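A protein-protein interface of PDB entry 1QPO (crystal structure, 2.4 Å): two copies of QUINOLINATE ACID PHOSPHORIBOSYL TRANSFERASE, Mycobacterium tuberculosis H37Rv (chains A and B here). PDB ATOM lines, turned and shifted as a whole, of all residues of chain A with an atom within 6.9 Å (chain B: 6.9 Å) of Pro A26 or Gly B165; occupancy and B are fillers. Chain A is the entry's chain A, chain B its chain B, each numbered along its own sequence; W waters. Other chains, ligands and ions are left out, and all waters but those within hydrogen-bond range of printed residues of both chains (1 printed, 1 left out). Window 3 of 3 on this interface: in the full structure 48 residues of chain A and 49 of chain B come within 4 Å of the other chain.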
ATOM      1  N   ASP A  21      22.211  23.006 -20.144  1.00  0.00           N
ATOM      2  CA  ASP A  21      20.849  23.290 -20.564  1.00  0.00           C
ATOM      3  C   ASP A  21      20.084  22.158 -21.206  1.00  0.00           C
ATOM      4  O   ASP A  21      18.846  22.122 -21.128  1.00  0.00           O
ATOM      5  CB  ASP A  21      20.846  24.473 -21.528  1.00  0.00           C
ATOM      6  CG  ASP A  21      20.081  25.671 -20.991  1.00  0.00           C
ATOM      7  OD1 ASP A  21      19.636  25.662 -19.819  1.00  0.00           O
ATOM      8  OD2 ASP A  21      19.927  26.642 -21.747  1.00  0.00           O
ATOM      9  N   LEU A  22      20.806  21.265 -21.884  1.00  0.00           N
ATOM     10  CA  LEU A  22      20.184  20.165 -22.619  1.00  0.00           C
ATOM     11  C   LEU A  22      20.298  18.826 -21.951  1.00  0.00           C
ATOM     12  O   LEU A  22      19.755  17.850 -22.432  1.00  0.00           O
ATOM     13  CB  LEU A  22      20.732  20.115 -24.050  1.00  0.00           C
ATOM     14  CG  LEU A  22      20.401  21.368 -24.865  1.00  0.00           C
ATOM     15  CD1 LEU A  22      21.199  21.391 -26.076  1.00  0.00           C
ATOM     16  CD2 LEU A  22      18.944  21.436 -25.219  1.00  0.00           C
ATOM     17  N   ARG A  23      20.948  18.798 -20.803  1.00  0.00           N
ATOM     18  CA  ARG A  23      21.133  17.575 -20.053  1.00  0.00           C
ATOM     19  C   ARG A  23      19.836  16.878 -19.633  1.00  0.00           C
ATOM     20  O   ARG A  23      19.827  15.680 -19.423  1.00  0.00           O
ATOM     21  CB  ARG A  23      21.950  17.890 -18.799  1.00  0.00           C
ATOM     22  CG  ARG A  23      22.208  16.689 -17.893  1.00  0.00           C
ATOM     23  CD  ARG A  23      22.933  17.085 -16.618  1.00  0.00           C
ATOM     24  NE  ARG A  23      23.972  18.072 -16.899  1.00  0.00           N
ATOM     25  CZ  ARG A  23      25.043  17.853 -17.665  1.00  0.00           C
ATOM     26  NH1 ARG A  23      25.240  16.660 -18.246  1.00  0.00           N
ATOM     27  NH2 ARG A  23      25.927  18.839 -17.844  1.00  0.00           N
ATOM     28  N   TYR A  24      18.740  17.618 -19.501  1.00  0.00           N
ATOM     29  CA  TYR A  24      17.490  17.023 -19.036  1.00  0.00           C
ATOM     30  C   TYR A  24      16.452  16.805 -20.102  1.00  0.00           C
ATOM     31  O   TYR A  24      15.348  16.384 -19.798  1.00  0.00           O
ATOM     32  CB  TYR A  24      16.893  17.865 -17.896  1.00  0.00           C
ATOM     33  CG  TYR A  24      17.914  18.181 -16.845  1.00  0.00           C
ATOM     34  CD1 TYR A  24      18.814  19.232 -17.027  1.00  0.00           C
ATOM     35  CD2 TYR A  24      18.076  17.350 -15.735  1.00  0.00           C
ATOM     36  CE1 TYR A  24      19.865  19.440 -16.137  1.00  0.00           C
ATOM     37  CE2 TYR A  24      19.121  17.542 -14.831  1.00  0.00           C
ATOM     38  CZ  TYR A  24      20.020  18.589 -15.041  1.00  0.00           C
ATOM     39  OH  TYR A  24      21.097  18.758 -14.184  1.00  0.00           O
ATOM     40  N   GLY A  25      16.781  17.072 -21.354  1.00  0.00           N
ATOM     41  CA  GLY A  25      15.791  16.876 -22.399  1.00  0.00           C
ATOM     42  C   GLY A  25      15.643  18.144 -23.209  1.00  0.00           C
ATOM     43  O   GLY A  25      15.989  19.227 -22.715  1.00  0.00           O
ATOM     44  N   PRO A  26      15.117  18.063 -24.447  1.00  0.00           N
ATOM     45  CA  PRO A  26      14.959  19.254 -25.279  1.00  0.00           C
ATOM     46  C   PRO A  26      13.839  20.126 -24.774  1.00  0.00           C
ATOM     47  O   PRO A  26      13.096  19.756 -23.867  1.00  0.00           O
ATOM     48  CB  PRO A  26      14.640  18.668 -26.646  1.00  0.00           C
ATOM     49  CG  PRO A  26      13.784  17.510 -26.274  1.00  0.00           C
ATOM     50  CD  PRO A  26      14.507  16.889 -25.096  1.00  0.00           C
ATOM     51  N   ASP A  27      13.751  21.308 -25.348  1.00  0.00           N
ATOM     52  CA  ASP A  27      12.726  22.249 -24.983  1.00  0.00           C
ATOM     53  C   ASP A  27      11.399  21.757 -25.554  1.00  0.00           C
ATOM     54  O   ASP A  27      10.969  22.183 -26.625  1.00  0.00           O
ATOM     55  CB  ASP A  27      13.081  23.588 -25.574  1.00  0.00           C
ATOM     56  CG  ASP A  27      12.259  24.691 -25.021  1.00  0.00           C
ATOM     57  OD1 ASP A  27      11.275  24.428 -24.290  1.00  0.00           O
ATOM     58  OD2 ASP A  27      12.614  25.852 -25.319  1.00  0.00           O
ATOM     59  N   VAL A  28      10.757  20.863 -24.815  1.00  0.00           N
ATOM     60  CA  VAL A  28       9.497  20.261 -25.197  1.00  0.00           C
ATOM     61  C   VAL A  28       8.421  21.259 -25.568  1.00  0.00           C
ATOM     62  O   VAL A  28       7.573  20.986 -26.408  1.00  0.00           O
ATOM     63  CB  VAL A  28       9.012  19.340 -24.082  1.00  0.00           C
ATOM     64  CG1 VAL A  28       9.148  20.028 -22.764  1.00  0.00           C
ATOM     65  CG2 VAL A  28       7.575  18.941 -24.305  1.00  0.00           C
ATOM     66  N   THR A  29       8.465  22.445 -24.987  1.00  0.00           N
ATOM     67  CA  THR A  29       7.451  23.421 -25.319  1.00  0.00           C
ATOM     68  C   THR A  29       7.627  24.039 -26.698  1.00  0.00           C
ATOM     69  O   THR A  29       6.645  24.204 -27.399  1.00  0.00           O
ATOM     70  CB  THR A  29       7.221  24.466 -24.167  1.00  0.00           C
ATOM     71  OG1 THR A  29       6.518  25.617 -24.659  1.00  0.00           O
ATOM     72  CG2 THR A  29       8.523  24.879 -23.512  1.00  0.00           C
ATOM     73  N   LEU A  31       9.093  22.588 -29.160  1.00  0.00           N
ATOM     74  CA  LEU A  31       8.903  21.460 -30.076  1.00  0.00           C
ATOM     75  C   LEU A  31       7.422  21.333 -30.333  1.00  0.00           C
ATOM     76  O   LEU A  31       7.003  21.171 -31.466  1.00  0.00           O
ATOM     77  CB  LEU A  31       9.415  20.154 -29.467  1.00  0.00           C
ATOM     78  CG  LEU A  31      10.841  19.785 -29.834  1.00  0.00           C
ATOM     79  CD1 LEU A  31      11.748  20.983 -29.654  1.00  0.00           C
ATOM     80  CD2 LEU A  31      11.311  18.614 -28.982  1.00  0.00           C
ATOM     81  N   THR A 101      16.610  27.677 -28.325  1.00  0.00           N
ATOM     82  CA  THR A 101      17.457  26.715 -27.625  1.00  0.00           C
ATOM     83  C   THR A 101      18.772  27.374 -27.235  1.00  0.00           C
ATOM     84  O   THR A 101      19.261  27.146 -26.129  1.00  0.00           O
ATOM     85  CB  THR A 101      17.737  25.451 -28.491  1.00  0.00           C
ATOM     86  OG1 THR A 101      16.535  24.666 -28.570  1.00  0.00           O
ATOM     87  CG2 THR A 101      18.866  24.596 -27.881  1.00  0.00           C
ATOM     88  N   ARG B 138      17.954  30.077 -14.414  1.00  0.00           N
ATOM     89  CA  ARG B 138      18.885  29.474 -15.377  1.00  0.00           C
ATOM     90  C   ARG B 138      19.889  30.546 -15.844  1.00  0.00           C
ATOM     91  O   ARG B 138      20.658  30.309 -16.775  1.00  0.00           O
ATOM     92  CB  ARG B 138      18.164  28.892 -16.598  1.00  0.00           C
ATOM     93  CG  ARG B 138      17.430  27.567 -16.339  1.00  0.00           C
ATOM     94  CD  ARG B 138      17.177  26.817 -17.642  1.00  0.00           C
ATOM     95  NE  ARG B 138      16.369  27.620 -18.536  1.00  0.00           N
ATOM     96  CZ  ARG B 138      16.722  27.968 -19.759  1.00  0.00           C
ATOM     97  NH1 ARG B 138      17.866  27.579 -20.246  1.00  0.00           N
ATOM     98  NH2 ARG B 138      15.950  28.769 -20.474  1.00  0.00           N
ATOM     99  N   ARG B 161      14.657  25.771 -12.139  1.00  0.00           N
ATOM    100  CA  ARG B 161      14.904  24.915 -13.281  1.00  0.00           C
ATOM    101  C   ARG B 161      16.381  24.584 -13.474  1.00  0.00           C
ATOM    102  O   ARG B 161      17.227  25.461 -13.354  1.00  0.00           O
ATOM    103  CB  ARG B 161      14.270  25.527 -14.539  1.00  0.00           C
ATOM    104  CG  ARG B 161      12.803  25.133 -14.735  1.00  0.00           C
ATOM    105  CD  ARG B 161      12.503  24.690 -16.168  1.00  0.00           C
ATOM    106  NE  ARG B 161      12.516  25.819 -17.080  1.00  0.00           N
ATOM    107  CZ  ARG B 161      12.567  25.717 -18.400  1.00  0.00           C
ATOM    108  NH1 ARG B 161      12.604  24.526 -18.967  1.00  0.00           N
ATOM    109  NH2 ARG B 161      12.607  26.810 -19.164  1.00  0.00           N
ATOM    110  N   LEU B 162      16.696  23.313 -13.706  1.00  0.00           N
ATOM    111  CA  LEU B 162      18.087  22.921 -13.906  1.00  0.00           C
ATOM    112  C   LEU B 162      18.481  22.969 -15.359  1.00  0.00           C
ATOM    113  O   LEU B 162      19.671  23.086 -15.681  1.00  0.00           O
ATOM    114  CB  LEU B 162      18.371  21.531 -13.338  1.00  0.00           C
ATOM    115  CG  LEU B 162      18.379  21.355 -11.807  1.00  0.00           C
ATOM    116  CD1 LEU B 162      18.832  19.926 -11.478  1.00  0.00           C
ATOM    117  CD2 LEU B 162      19.295  22.360 -11.152  1.00  0.00           C
ATOM    118  N   GLY B 163      17.472  22.957 -16.227  1.00  0.00           N
ATOM    119  CA  GLY B 163      17.710  23.005 -17.653  1.00  0.00           C
ATOM    120  C   GLY B 163      16.456  23.209 -18.475  1.00  0.00           C
ATOM    121  O   GLY B 163      15.372  23.384 -17.943  1.00  0.00           O
ATOM    122  N   LEU B 164      16.594  23.116 -19.785  1.00  0.00           N
ATOM    123  CA  LEU B 164      15.476  23.318 -20.693  1.00  0.00           C
ATOM    124  C   LEU B 164      14.394  22.281 -20.631  1.00  0.00           C
ATOM    125  O   LEU B 164      13.242  22.593 -20.818  1.00  0.00           O
ATOM    126  CB  LEU B 164      15.992  23.357 -22.118  1.00  0.00           C
ATOM    127  CG  LEU B 164      15.975  24.643 -22.924  1.00  0.00           C
ATOM    128  CD1 LEU B 164      15.756  25.791 -22.040  1.00  0.00           C
ATOM    129  CD2 LEU B 164      17.238  24.803 -23.720  1.00  0.00           C
ATOM    130  N   GLY B 165      14.770  21.035 -20.420  1.00  0.00           N
ATOM    131  CA  GLY B 165      13.784  19.971 -20.421  1.00  0.00           C
ATOM    132  C   GLY B 165      13.210  19.684 -19.070  1.00  0.00           C
ATOM    133  O   GLY B 165      12.319  18.857 -18.917  1.00  0.00           O
ATOM    134  N   ASP B 166      13.767  20.386 -18.096  1.00  0.00           N
ATOM    135  CA  ASP B 166      13.413  20.320 -16.685  1.00  0.00           C
ATOM    136  C   ASP B 166      11.898  20.452 -16.376  1.00  0.00           C
ATOM    137  O   ASP B 166      11.377  19.782 -15.487  1.00  0.00           O
ATOM    138  CB  ASP B 166      14.160  21.473 -16.003  1.00  0.00           C
ATOM    139  CG  ASP B 166      14.499  21.176 -14.596  1.00  0.00           C
ATOM    140  OD1 ASP B 166      15.305  20.250 -14.370  1.00  0.00           O
ATOM    141  OD2 ASP B 166      13.960  21.856 -13.702  1.00  0.00           O
ATOM    142  N   ALA B 167      11.233  21.382 -17.058  1.00  0.00           N
ATOM    143  CA  ALA B 167       9.822  21.678 -16.863  1.00  0.00           C
ATOM    144  C   ALA B 167       9.384  22.421 -18.124  1.00  0.00           C
ATOM    145  O   ALA B 167      10.231  22.854 -18.900  1.00  0.00           O
ATOM    146  CB  ALA B 167       9.648  22.587 -15.643  1.00  0.00           C
ATOM    147  N   ALA B 168       8.082  22.507 -18.373  1.00  0.00           N
ATOM    148  CA  ALA B 168       7.593  23.213 -19.558  1.00  0.00           C
ATOM    149  C   ALA B 168       7.302  24.662 -19.166  1.00  0.00           C
ATOM    150  O   ALA B 168       6.559  24.934 -18.217  1.00  0.00           O
ATOM    151  CB  ALA B 168       6.344  22.545 -20.111  1.00  0.00           C
ATOM    152  N   LEU B 195       4.849  16.580 -17.247  1.00  0.00           N
ATOM    153  CA  LEU B 195       5.762  17.671 -16.955  1.00  0.00           C
ATOM    154  C   LEU B 195       5.122  18.890 -16.300  1.00  0.00           C
ATOM    155  O   LEU B 195       4.032  19.321 -16.704  1.00  0.00           O
ATOM    156  CB  LEU B 195       6.411  18.099 -18.262  1.00  0.00           C
ATOM    157  CG  LEU B 195       7.892  18.412 -18.216  1.00  0.00           C
ATOM    158  CD1 LEU B 195       8.653  17.352 -17.422  1.00  0.00           C
ATOM    159  CD2 LEU B 195       8.397  18.502 -19.645  1.00  0.00           C
ATOM    160  N   PRO B 196       5.799  19.464 -15.281  1.00  0.00           N
ATOM    161  CA  PRO B 196       5.323  20.656 -14.554  1.00  0.00           C
ATOM    162  C   PRO B 196       5.165  21.775 -15.577  1.00  0.00           C
ATOM    163  O   PRO B 196       6.080  22.045 -16.358  1.00  0.00           O
ATOM    164  CB  PRO B 196       6.465  20.957 -13.594  1.00  0.00           C
ATOM    165  CG  PRO B 196       7.018  19.591 -13.309  1.00  0.00           C
ATOM    166  CD  PRO B 196       7.030  18.931 -14.672  1.00  0.00           C
HETATM  167  O   HOH W   1      22.076  21.692 -15.743  1.00  0.00           O
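Among the printed residues, pairs that only touch across the chains: Pro A26 with Gly B165 (3.5 Å), Val A28 with Leu B195 (3.6 Å), Tyr A24 with Leu B162 (3.7 Å), Asp A21 with Gly B163 (3.7 Å), Thr A101 with Leu B164 (3.9 Å), Tyr A24 with Gly B165 (3.96 Å) and Tyr A24 with Gly B163 (3.98 Å).
No position is printed for both chains.
The backbone carbonyl oxygen (O) of Gly B163 sits at hydrogen-bond distance from the guanidinium group (NH1) of Arg B161.
OD2 of Asp B166 lies within hydrogen-bond range of N of Leu B162 (3.1 Å).
NH1 of Arg B161 lies within hydrogen-bond range of O of Leu B164.
Among the printed residues, Asp or Glu carboxylates within 4 Å of a Lys or Arg side-chain nitrogen of the other chain: Asp A21 with Arg B138.
Water W1 lies within hydrogen-bond range of the backbone carbonyl oxygen (O) of Leu B162 (2.8 Å) and the side-chain hydroxyl (OH) of Tyr A24 (3.5 Å).
O of Gly A25 is in hydrogen-bond range of N of Gly B165, at 3.2 Å.
The side-chain carboxylate of Asp A21 lies within salt-bridge range of the guanidinium group of Arg B138 (2.6 Å).
The backbone carbonyl oxygen (O) of Asp A21 sits at hydrogen-bond distance from the backbone NH (N) of Leu B164 (2.8 Å).
Of the printed residues of chain B, Gly A25 touches Gly B165.
Pro A26 touches just one residue of chain B: Gly B165.
Asp A27 touches none of the printed residues of chain B.
Leu A31 touches none of the printed residues of chain B.
Of the printed residues of chain B, Thr A101 touches Leu B164.
Of the printed residues of chain A, Arg B138 touches Asp A21.
Of the printed residues of chain A, Leu B162 touches Tyr A24.
Of chain A, only Tyr A24, Gly A25 and Pro A26 come within 4 Å of Gly B165.
Of the printed residues of chain A, Leu B195 touches Val A28.
The nearest residue of chain B that does not touch Pro A26 is Leu B164 (4.2 Å).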
